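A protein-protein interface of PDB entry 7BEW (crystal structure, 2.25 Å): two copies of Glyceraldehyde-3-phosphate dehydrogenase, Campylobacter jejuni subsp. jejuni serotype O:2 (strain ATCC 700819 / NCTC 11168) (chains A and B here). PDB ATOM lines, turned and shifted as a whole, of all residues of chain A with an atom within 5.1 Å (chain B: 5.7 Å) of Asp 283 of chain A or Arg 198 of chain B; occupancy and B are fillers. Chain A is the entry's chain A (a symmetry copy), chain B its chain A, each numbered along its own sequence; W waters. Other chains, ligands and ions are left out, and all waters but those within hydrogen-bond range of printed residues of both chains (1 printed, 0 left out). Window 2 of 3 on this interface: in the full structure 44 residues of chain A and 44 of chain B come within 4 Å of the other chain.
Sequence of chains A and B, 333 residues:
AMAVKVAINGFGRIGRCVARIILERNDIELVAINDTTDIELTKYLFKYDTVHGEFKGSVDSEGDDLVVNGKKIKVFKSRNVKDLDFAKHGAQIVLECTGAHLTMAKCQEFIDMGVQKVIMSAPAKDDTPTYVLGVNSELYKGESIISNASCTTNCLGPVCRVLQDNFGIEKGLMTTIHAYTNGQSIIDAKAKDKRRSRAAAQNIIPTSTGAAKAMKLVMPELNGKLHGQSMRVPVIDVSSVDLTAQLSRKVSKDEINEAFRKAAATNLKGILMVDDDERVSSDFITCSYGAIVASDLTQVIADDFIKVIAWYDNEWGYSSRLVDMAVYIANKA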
ATOM      1  N   ARG A 279     -20.303  23.622 -13.756  1.00  0.00           N
ATOM      2  CA  ARG A 279     -19.445  23.824 -14.927  1.00  0.00           C
ATOM      3  C   ARG A 279     -19.243  22.487 -15.622  1.00  0.00           C
ATOM      4  O   ARG A 279     -19.556  21.413 -15.015  1.00  0.00           O
ATOM      5  CB  ARG A 279     -18.122  24.461 -14.515  1.00  0.00           C
ATOM      6  CG  ARG A 279     -18.263  25.954 -14.234  1.00  0.00           C
ATOM      7  CD  ARG A 279     -16.998  26.564 -13.681  1.00  0.00           C
ATOM      8  NE  ARG A 279     -17.060  26.528 -12.221  1.00  0.00           N
ATOM      9  CZ  ARG A 279     -16.259  27.206 -11.390  1.00  0.00           C
ATOM     10  NH1 ARG A 279     -15.296  27.990 -11.854  1.00  0.00           N
ATOM     11  NH2 ARG A 279     -16.469  27.124 -10.090  1.00  0.00           N
ATOM     12  N   VAL A 280     -18.760  22.587 -16.856  1.00  0.00           N
ATOM     13  CA  VAL A 280     -18.363  21.444 -17.717  1.00  0.00           C
ATOM     14  C   VAL A 280     -16.864  21.577 -17.991  1.00  0.00           C
ATOM     15  O   VAL A 280     -16.280  22.579 -17.567  1.00  0.00           O
ATOM     16  CB  VAL A 280     -19.223  21.431 -18.991  1.00  0.00           C
ATOM     17  CG1 VAL A 280     -20.685  21.226 -18.627  1.00  0.00           C
ATOM     18  CG2 VAL A 280     -19.067  22.694 -19.799  1.00  0.00           C
ATOM     19  N   SER A 281     -16.254  20.609 -18.677  1.00  0.00           N
ATOM     20  CA  SER A 281     -14.780  20.505 -18.739  1.00  0.00           C
ATOM     21  C   SER A 281     -14.153  21.807 -19.265  1.00  0.00           C
ATOM     22  O   SER A 281     -13.154  22.274 -18.671  1.00  0.00           O
ATOM     23  CB  SER A 281     -14.360  19.289 -19.513  1.00  0.00           C
ATOM     24  OG  SER A 281     -14.938  19.276 -20.801  1.00  0.00           O
ATOM     25  N   SER A 282     -14.658  22.366 -20.363  1.00  0.00           N
ATOM     26  CA  SER A 282     -14.011  23.517 -21.039  1.00  0.00           C
ATOM     27  C   SER A 282     -13.963  24.738 -20.104  1.00  0.00           C
ATOM     28  O   SER A 282     -13.104  25.642 -20.320  1.00  0.00           O
ATOM     29  CB  SER A 282     -14.664  23.827 -22.361  1.00  0.00           C
ATOM     30  OG  SER A 282     -15.932  24.408 -22.112  1.00  0.00           O
ATOM     31  N   ASP A 283     -14.794  24.767 -19.058  1.00  0.00           N
ATOM     32  CA  ASP A 283     -14.792  25.890 -18.097  1.00  0.00           C
ATOM     33  C   ASP A 283     -13.500  25.895 -17.287  1.00  0.00           C
ATOM     34  O   ASP A 283     -13.220  26.935 -16.680  1.00  0.00           O
ATOM     35  CB  ASP A 283     -16.010  25.834 -17.177  1.00  0.00           C
ATOM     36  CG  ASP A 283     -17.303  26.014 -17.937  1.00  0.00           C
ATOM     37  OD1 ASP A 283     -17.285  26.830 -18.922  1.00  0.00           O
ATOM     38  OD2 ASP A 283     -18.298  25.336 -17.566  1.00  0.00           O
ATOM     39  N   PHE A 284     -12.783  24.778 -17.215  1.00  0.00           N
ATOM     40  CA  PHE A 284     -11.557  24.635 -16.396  1.00  0.00           C
ATOM     41  C   PHE A 284     -10.293  24.704 -17.242  1.00  0.00           C
ATOM     42  O   PHE A 284      -9.206  24.474 -16.678  1.00  0.00           O
ATOM     43  CB  PHE A 284     -11.643  23.342 -15.596  1.00  0.00           C
ATOM     44  CG  PHE A 284     -12.829  23.387 -14.683  1.00  0.00           C
ATOM     45  CD1 PHE A 284     -12.861  24.302 -13.642  1.00  0.00           C
ATOM     46  CD2 PHE A 284     -13.928  22.586 -14.921  1.00  0.00           C
ATOM     47  CE1 PHE A 284     -13.979  24.404 -12.840  1.00  0.00           C
ATOM     48  CE2 PHE A 284     -15.034  22.655 -14.097  1.00  0.00           C
ATOM     49  CZ  PHE A 284     -15.057  23.560 -13.057  1.00  0.00           C
ATOM     50  N   ILE A 285     -10.406  25.087 -18.518  1.00  0.00           N
ATOM     51  CA  ILE A 285      -9.215  25.277 -19.381  1.00  0.00           C
ATOM     52  C   ILE A 285      -8.442  26.466 -18.816  1.00  0.00           C
ATOM     53  O   ILE A 285      -9.036  27.523 -18.602  1.00  0.00           O
ATOM     54  CB  ILE A 285      -9.596  25.427 -20.861  1.00  0.00           C
ATOM     55  CG1 ILE A 285     -10.118  24.100 -21.425  1.00  0.00           C
ATOM     56  CG2 ILE A 285      -8.412  25.944 -21.667  1.00  0.00           C
ATOM     57  CD1 ILE A 285     -10.789  24.255 -22.775  1.00  0.00           C
ATOM     58  N   GLN B 184     -29.114  16.971 -26.719  1.00  0.00           N
ATOM     59  CA  GLN B 184     -27.901  17.683 -26.255  1.00  0.00           C
ATOM     60  C   GLN B 184     -27.638  18.777 -27.302  1.00  0.00           C
ATOM     61  O   GLN B 184     -27.909  18.496 -28.487  1.00  0.00           O
ATOM     62  CB  GLN B 184     -26.743  16.699 -26.117  1.00  0.00           C
ATOM     63  CG  GLN B 184     -26.543  16.155 -24.710  1.00  0.00           C
ATOM     64  CD  GLN B 184     -25.189  15.500 -24.585  1.00  0.00           C
ATOM     65  OE1 GLN B 184     -25.000  14.353 -24.970  1.00  0.00           O
ATOM     66  NE2 GLN B 184     -24.222  16.228 -24.057  1.00  0.00           N
ATOM     67  N   SER B 185     -27.174  19.973 -26.913  1.00  0.00           N
ATOM     68  CA  SER B 185     -26.901  21.083 -27.864  1.00  0.00           C
ATOM     69  C   SER B 185     -25.521  20.930 -28.503  1.00  0.00           C
ATOM     70  O   SER B 185     -24.566  20.542 -27.838  1.00  0.00           O
ATOM     71  CB  SER B 185     -27.071  22.481 -27.296  1.00  0.00           C
ATOM     72  OG  SER B 185     -27.124  22.503 -25.878  1.00  0.00           O
ATOM     73  N   ILE B 186     -25.488  21.275 -29.779  1.00  0.00           N
ATOM     74  CA  ILE B 186     -24.306  21.360 -30.671  1.00  0.00           C
ATOM     75  C   ILE B 186     -23.428  22.534 -30.199  1.00  0.00           C
ATOM     76  O   ILE B 186     -22.206  22.422 -30.277  1.00  0.00           O
ATOM     77  CB  ILE B 186     -24.819  21.501 -32.124  1.00  0.00           C
ATOM     78  CG1 ILE B 186     -23.709  21.428 -33.173  1.00  0.00           C
ATOM     79  CG2 ILE B 186     -25.628  22.782 -32.298  1.00  0.00           C
ATOM     80  CD1 ILE B 186     -22.808  20.227 -33.031  1.00  0.00           C
ATOM     81  N   ILE B 187     -24.037  23.640 -29.769  1.00  0.00           N
ATOM     82  CA  ILE B 187     -23.326  24.877 -29.341  1.00  0.00           C
ATOM     83  C   ILE B 187     -23.926  25.263 -27.993  1.00  0.00           C
ATOM     84  O   ILE B 187     -24.949  24.687 -27.628  1.00  0.00           O
ATOM     85  CB  ILE B 187     -23.427  26.018 -30.380  1.00  0.00           C
ATOM     86  CG1 ILE B 187     -24.839  26.210 -30.922  1.00  0.00           C
ATOM     87  CG2 ILE B 187     -22.436  25.842 -31.502  1.00  0.00           C
ATOM     88  CD1 ILE B 187     -25.821  26.747 -29.897  1.00  0.00           C
ATOM     89  N   ASP B 188     -23.304  26.156 -27.237  1.00  0.00           N
ATOM     90  CA  ASP B 188     -23.883  26.523 -25.918  1.00  0.00           C
ATOM     91  C   ASP B 188     -25.236  27.198 -26.196  1.00  0.00           C
ATOM     92  O   ASP B 188     -25.244  28.290 -26.807  1.00  0.00           O
ATOM     93  CB  ASP B 188     -22.956  27.428 -25.095  1.00  0.00           C
ATOM     94  CG  ASP B 188     -21.592  26.887 -24.676  1.00  0.00           C
ATOM     95  OD1 ASP B 188     -21.344  25.660 -24.696  1.00  0.00           O
ATOM     96  OD2 ASP B 188     -20.798  27.707 -24.228  1.00  0.00           O
ATOM     97  N   ALA B 189     -26.345  26.586 -25.784  1.00  0.00           N
ATOM     98  CA  ALA B 189     -27.706  27.117 -26.007  1.00  0.00           C
ATOM     99  C   ALA B 189     -28.659  26.505 -24.991  1.00  0.00           C
ATOM    100  O   ALA B 189     -28.445  25.354 -24.574  1.00  0.00           O
ATOM    101  CB  ALA B 189     -28.157  26.824 -27.415  1.00  0.00           C
ATOM    102  N   LYS B 194     -28.605  23.392 -16.868  1.00  0.00           N
ATOM    103  CA  LYS B 194     -27.347  24.115 -17.138  1.00  0.00           C
ATOM    104  C   LYS B 194     -26.422  23.270 -18.004  1.00  0.00           C
ATOM    105  O   LYS B 194     -26.108  23.699 -19.117  1.00  0.00           O
ATOM    106  CB  LYS B 194     -26.719  24.495 -15.810  1.00  0.00           C
ATOM    107  CG  LYS B 194     -27.421  25.648 -15.128  1.00  0.00           C
ATOM    108  CD  LYS B 194     -26.796  25.929 -13.822  1.00  0.00           C
ATOM    109  CE  LYS B 194     -27.456  27.033 -13.057  1.00  0.00           C
ATOM    110  NZ  LYS B 194     -26.652  27.261 -11.835  1.00  0.00           N
ATOM    111  N   ARG B 195     -25.998  22.121 -17.499  1.00  0.00           N
ATOM    112  CA  ARG B 195     -24.974  21.274 -18.155  1.00  0.00           C
ATOM    113  C   ARG B 195     -25.446  20.795 -19.537  1.00  0.00           C
ATOM    114  O   ARG B 195     -24.622  20.806 -20.470  1.00  0.00           O
ATOM    115  CB  ARG B 195     -24.573  20.152 -17.205  1.00  0.00           C
ATOM    116  CG  ARG B 195     -23.712  20.653 -16.057  1.00  0.00           C
ATOM    117  CD  ARG B 195     -22.780  19.587 -15.544  1.00  0.00           C
ATOM    118  NE  ARG B 195     -22.000  19.844 -14.323  1.00  0.00           N
ATOM    119  CZ  ARG B 195     -22.380  19.546 -13.076  1.00  0.00           C
ATOM    120  NH1 ARG B 195     -23.592  19.098 -12.824  1.00  0.00           N
ATOM    121  NH2 ARG B 195     -21.552  19.754 -12.069  1.00  0.00           N
ATOM    122  N   ARG B 196     -26.724  20.451 -19.689  1.00  0.00           N
ATOM    123  CA  ARG B 196     -27.286  20.011 -20.990  1.00  0.00           C
ATOM    124  C   ARG B 196     -27.262  21.180 -22.003  1.00  0.00           C
ATOM    125  O   ARG B 196     -27.329  20.910 -23.225  1.00  0.00           O
ATOM    126  CB  ARG B 196     -28.694  19.435 -20.793  1.00  0.00           C
ATOM    127  CG  ARG B 196     -28.920  18.128 -21.539  1.00  0.00           C
ATOM    128  CD  ARG B 196     -30.354  17.641 -21.503  1.00  0.00           C
ATOM    129  NE  ARG B 196     -30.869  17.550 -20.141  1.00  0.00           N
ATOM    130  CZ  ARG B 196     -32.162  17.458 -19.820  1.00  0.00           C
ATOM    131  NH1 ARG B 196     -33.095  17.433 -20.761  1.00  0.00           N
ATOM    132  NH2 ARG B 196     -32.522  17.398 -18.548  1.00  0.00           N
ATOM    133  N   SER B 197     -27.141  22.427 -21.537  1.00  0.00           N
ATOM    134  CA  SER B 197     -27.029  23.621 -22.412  1.00  0.00           C
ATOM    135  C   SER B 197     -25.656  23.718 -23.102  1.00  0.00           C
ATOM    136  O   SER B 197     -25.524  24.573 -24.014  1.00  0.00           O
ATOM    137  CB  SER B 197     -27.339  24.874 -21.657  1.00  0.00           C
ATOM    138  OG  SER B 197     -28.667  24.843 -21.153  1.00  0.00           O
ATOM    139  N   ARG B 198     -24.665  22.899 -22.732  1.00  0.00           N
ATOM    140  CA  ARG B 198     -23.271  23.179 -23.153  1.00  0.00           C
ATOM    141  C   ARG B 198     -22.911  22.309 -24.359  1.00  0.00           C
ATOM    142  O   ARG B 198     -23.513  21.276 -24.527  1.00  0.00           O
ATOM    143  CB  ARG B 198     -22.333  23.013 -21.958  1.00  0.00           C
ATOM    144  CG  ARG B 198     -22.721  23.884 -20.779  1.00  0.00           C
ATOM    145  CD  ARG B 198     -22.648  25.342 -21.110  1.00  0.00           C
ATOM    146  NE  ARG B 198     -21.283  25.679 -21.461  1.00  0.00           N
ATOM    147  CZ  ARG B 198     -20.307  25.897 -20.584  1.00  0.00           C
ATOM    148  NH1 ARG B 198     -20.551  25.866 -19.279  1.00  0.00           N
ATOM    149  NH2 ARG B 198     -19.089  26.161 -21.019  1.00  0.00           N
ATOM    150  N   ALA B 199     -21.988  22.775 -25.190  1.00  0.00           N
ATOM    151  CA  ALA B 199     -21.601  22.147 -26.476  1.00  0.00           C
ATOM    152  C   ALA B 199     -21.137  20.689 -26.258  1.00  0.00           C
ATOM    153  O   ALA B 199     -20.117  20.431 -25.577  1.00  0.00           O
ATOM    154  CB  ALA B 199     -20.538  22.995 -27.101  1.00  0.00           C
ATOM    155  N   ALA B 200     -21.849  19.742 -26.842  1.00  0.00           N
ATOM    156  CA  ALA B 200     -21.685  18.298 -26.591  1.00  0.00           C
ATOM    157  C   ALA B 200     -20.424  17.727 -27.256  1.00  0.00           C
ATOM    158  O   ALA B 200     -19.898  16.703 -26.742  1.00  0.00           O
ATOM    159  CB  ALA B 200     -22.926  17.564 -27.039  1.00  0.00           C
ATOM    160  N   ASN B 203     -17.022  19.122 -24.912  1.00  0.00           N
ATOM    161  CA  ASN B 203     -16.984  19.073 -23.422  1.00  0.00           C
ATOM    162  C   ASN B 203     -17.199  17.646 -22.908  1.00  0.00           C
ATOM    163  O   ASN B 203     -17.857  16.833 -23.591  1.00  0.00           O
ATOM    164  CB  ASN B 203     -18.057  19.963 -22.799  1.00  0.00           C
ATOM    165  CG  ASN B 203     -17.782  21.429 -22.971  1.00  0.00           C
ATOM    166  OD1 ASN B 203     -16.835  21.958 -22.379  1.00  0.00           O
ATOM    167  ND2 ASN B 203     -18.555  22.074 -23.822  1.00  0.00           N
ATOM    168  N   ILE B 205     -19.467  16.295 -20.056  1.00  0.00           N
ATOM    169  CA  ILE B 205     -20.709  16.887 -19.499  1.00  0.00           C
ATOM    170  C   ILE B 205     -21.312  15.903 -18.505  1.00  0.00           C
ATOM    171  O   ILE B 205     -21.919  14.915 -18.901  1.00  0.00           O
ATOM    172  CB  ILE B 205     -21.674  17.284 -20.634  1.00  0.00           C
ATOM    173  CG1 ILE B 205     -20.976  18.242 -21.619  1.00  0.00           C
ATOM    174  CG2 ILE B 205     -22.938  17.874 -20.068  1.00  0.00           C
ATOM    175  CD1 ILE B 205     -21.893  18.940 -22.563  1.00  0.00           C
HETATM  176  O   HOH W   1     -18.828  20.735 -12.463  1.00  0.00           O
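Asp 283 of chain A touches one residue of chain B.
Arg 198 of chain B touches just these residues of chain A: Val 280, Ser 282 and Asp 283.
Of the printed residues of chain B, Arg 279 of chain A touches Arg 195 (3.0 Å).
Printed residues of chain B within 4 Å of Val 280 of chain A: Arg 198 (3.5 Å) and Asn 203 (3.5 Å).
Of the printed residues of chain A, Asn 203 of chain B touches Val 280, Ser 281 and Ser 282.
Of the printed residues of chain B, Ser 281 of chain A touches Asn 203.
Of the printed residues of chain B, Ser 282 of chain A touches Arg 198 and Asn 203.
Ile 205 of chain B touches none of the printed residues of chain A.
Ala 189 of chain B touches none of the printed residues of chain A.
The nearest residue of chain B that does not touch Asp 283 of chain A is Asn 203 of chain B (4.8 Å).
The nearest residue of chain A that does not touch Arg 198 of chain B is Arg 279 of chain A (4.9 Å).
NE of Arg 195 of chain B is in hydrogen-bond range of O of Arg 279 of chain A (3.0 Å).
OD1 of Asp 283 of chain A is in salt-bridge range of NH2 of Arg 198 of chain B, at 2.8 Å.
OG of Ser 282 of chain A lies within hydrogen-bond range of OD1 of Asn 203 of chain B (2.6 Å).
Val 280 of chain A touches Arg 198 of chain B.
Val 280 of chain A touches Asn 203 of chain B (CG2 to OD1, 3.5 Å).
Ser 281 of chain A touches Asn 203 of chain B (OG to CA, 3.3 Å).
Arg 198 of chain B touches Ser 282 of chain A.
Of the 15 printed residues of chain B, 3 touch a printed residue of chain A.
Of the 7 printed residues of chain A, 5 touch a printed residue of chain B.
Hydrophobic or aromatic side chains of chain A that line the printed part of chain B: Val 280.
Among the printed residues, Asp or Glu carboxylates within 4 Å of a Lys or Arg side-chain nitrogen of the other chain: Asp 283 of chain A with Arg 198 of chain B.
No position is printed for both chains.
Of the 7 pairs that touch across the chains among the printed residues, none has its exchanged pair printed and touching as well.
The backbone NH (N) of Val 280 of chain A lies within hydrogen-bond range of the side-chain carboxylate (OD2) of Asp 283 of chain A (2.9 Å).
The side-chain carboxylate (OD1) of Asp 188 of chain B lies within salt-bridge range of the guanidinium group (NE) of Arg 198 of chain B (3.2 Å).
The backbone carbonyl oxygen (O) of Ala 199 of chain B sits at hydrogen-bond distance from the side-chain amide nitrogen (ND2) of Asn 203 of chain B, at 2.9 Å.
Water W1 lies within hydrogen-bond range of the backbone carbonyl oxygen of Arg 279 of chain A (2.7 Å) and the guanidinium group of Arg 195 of chain B (2.9 Å).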
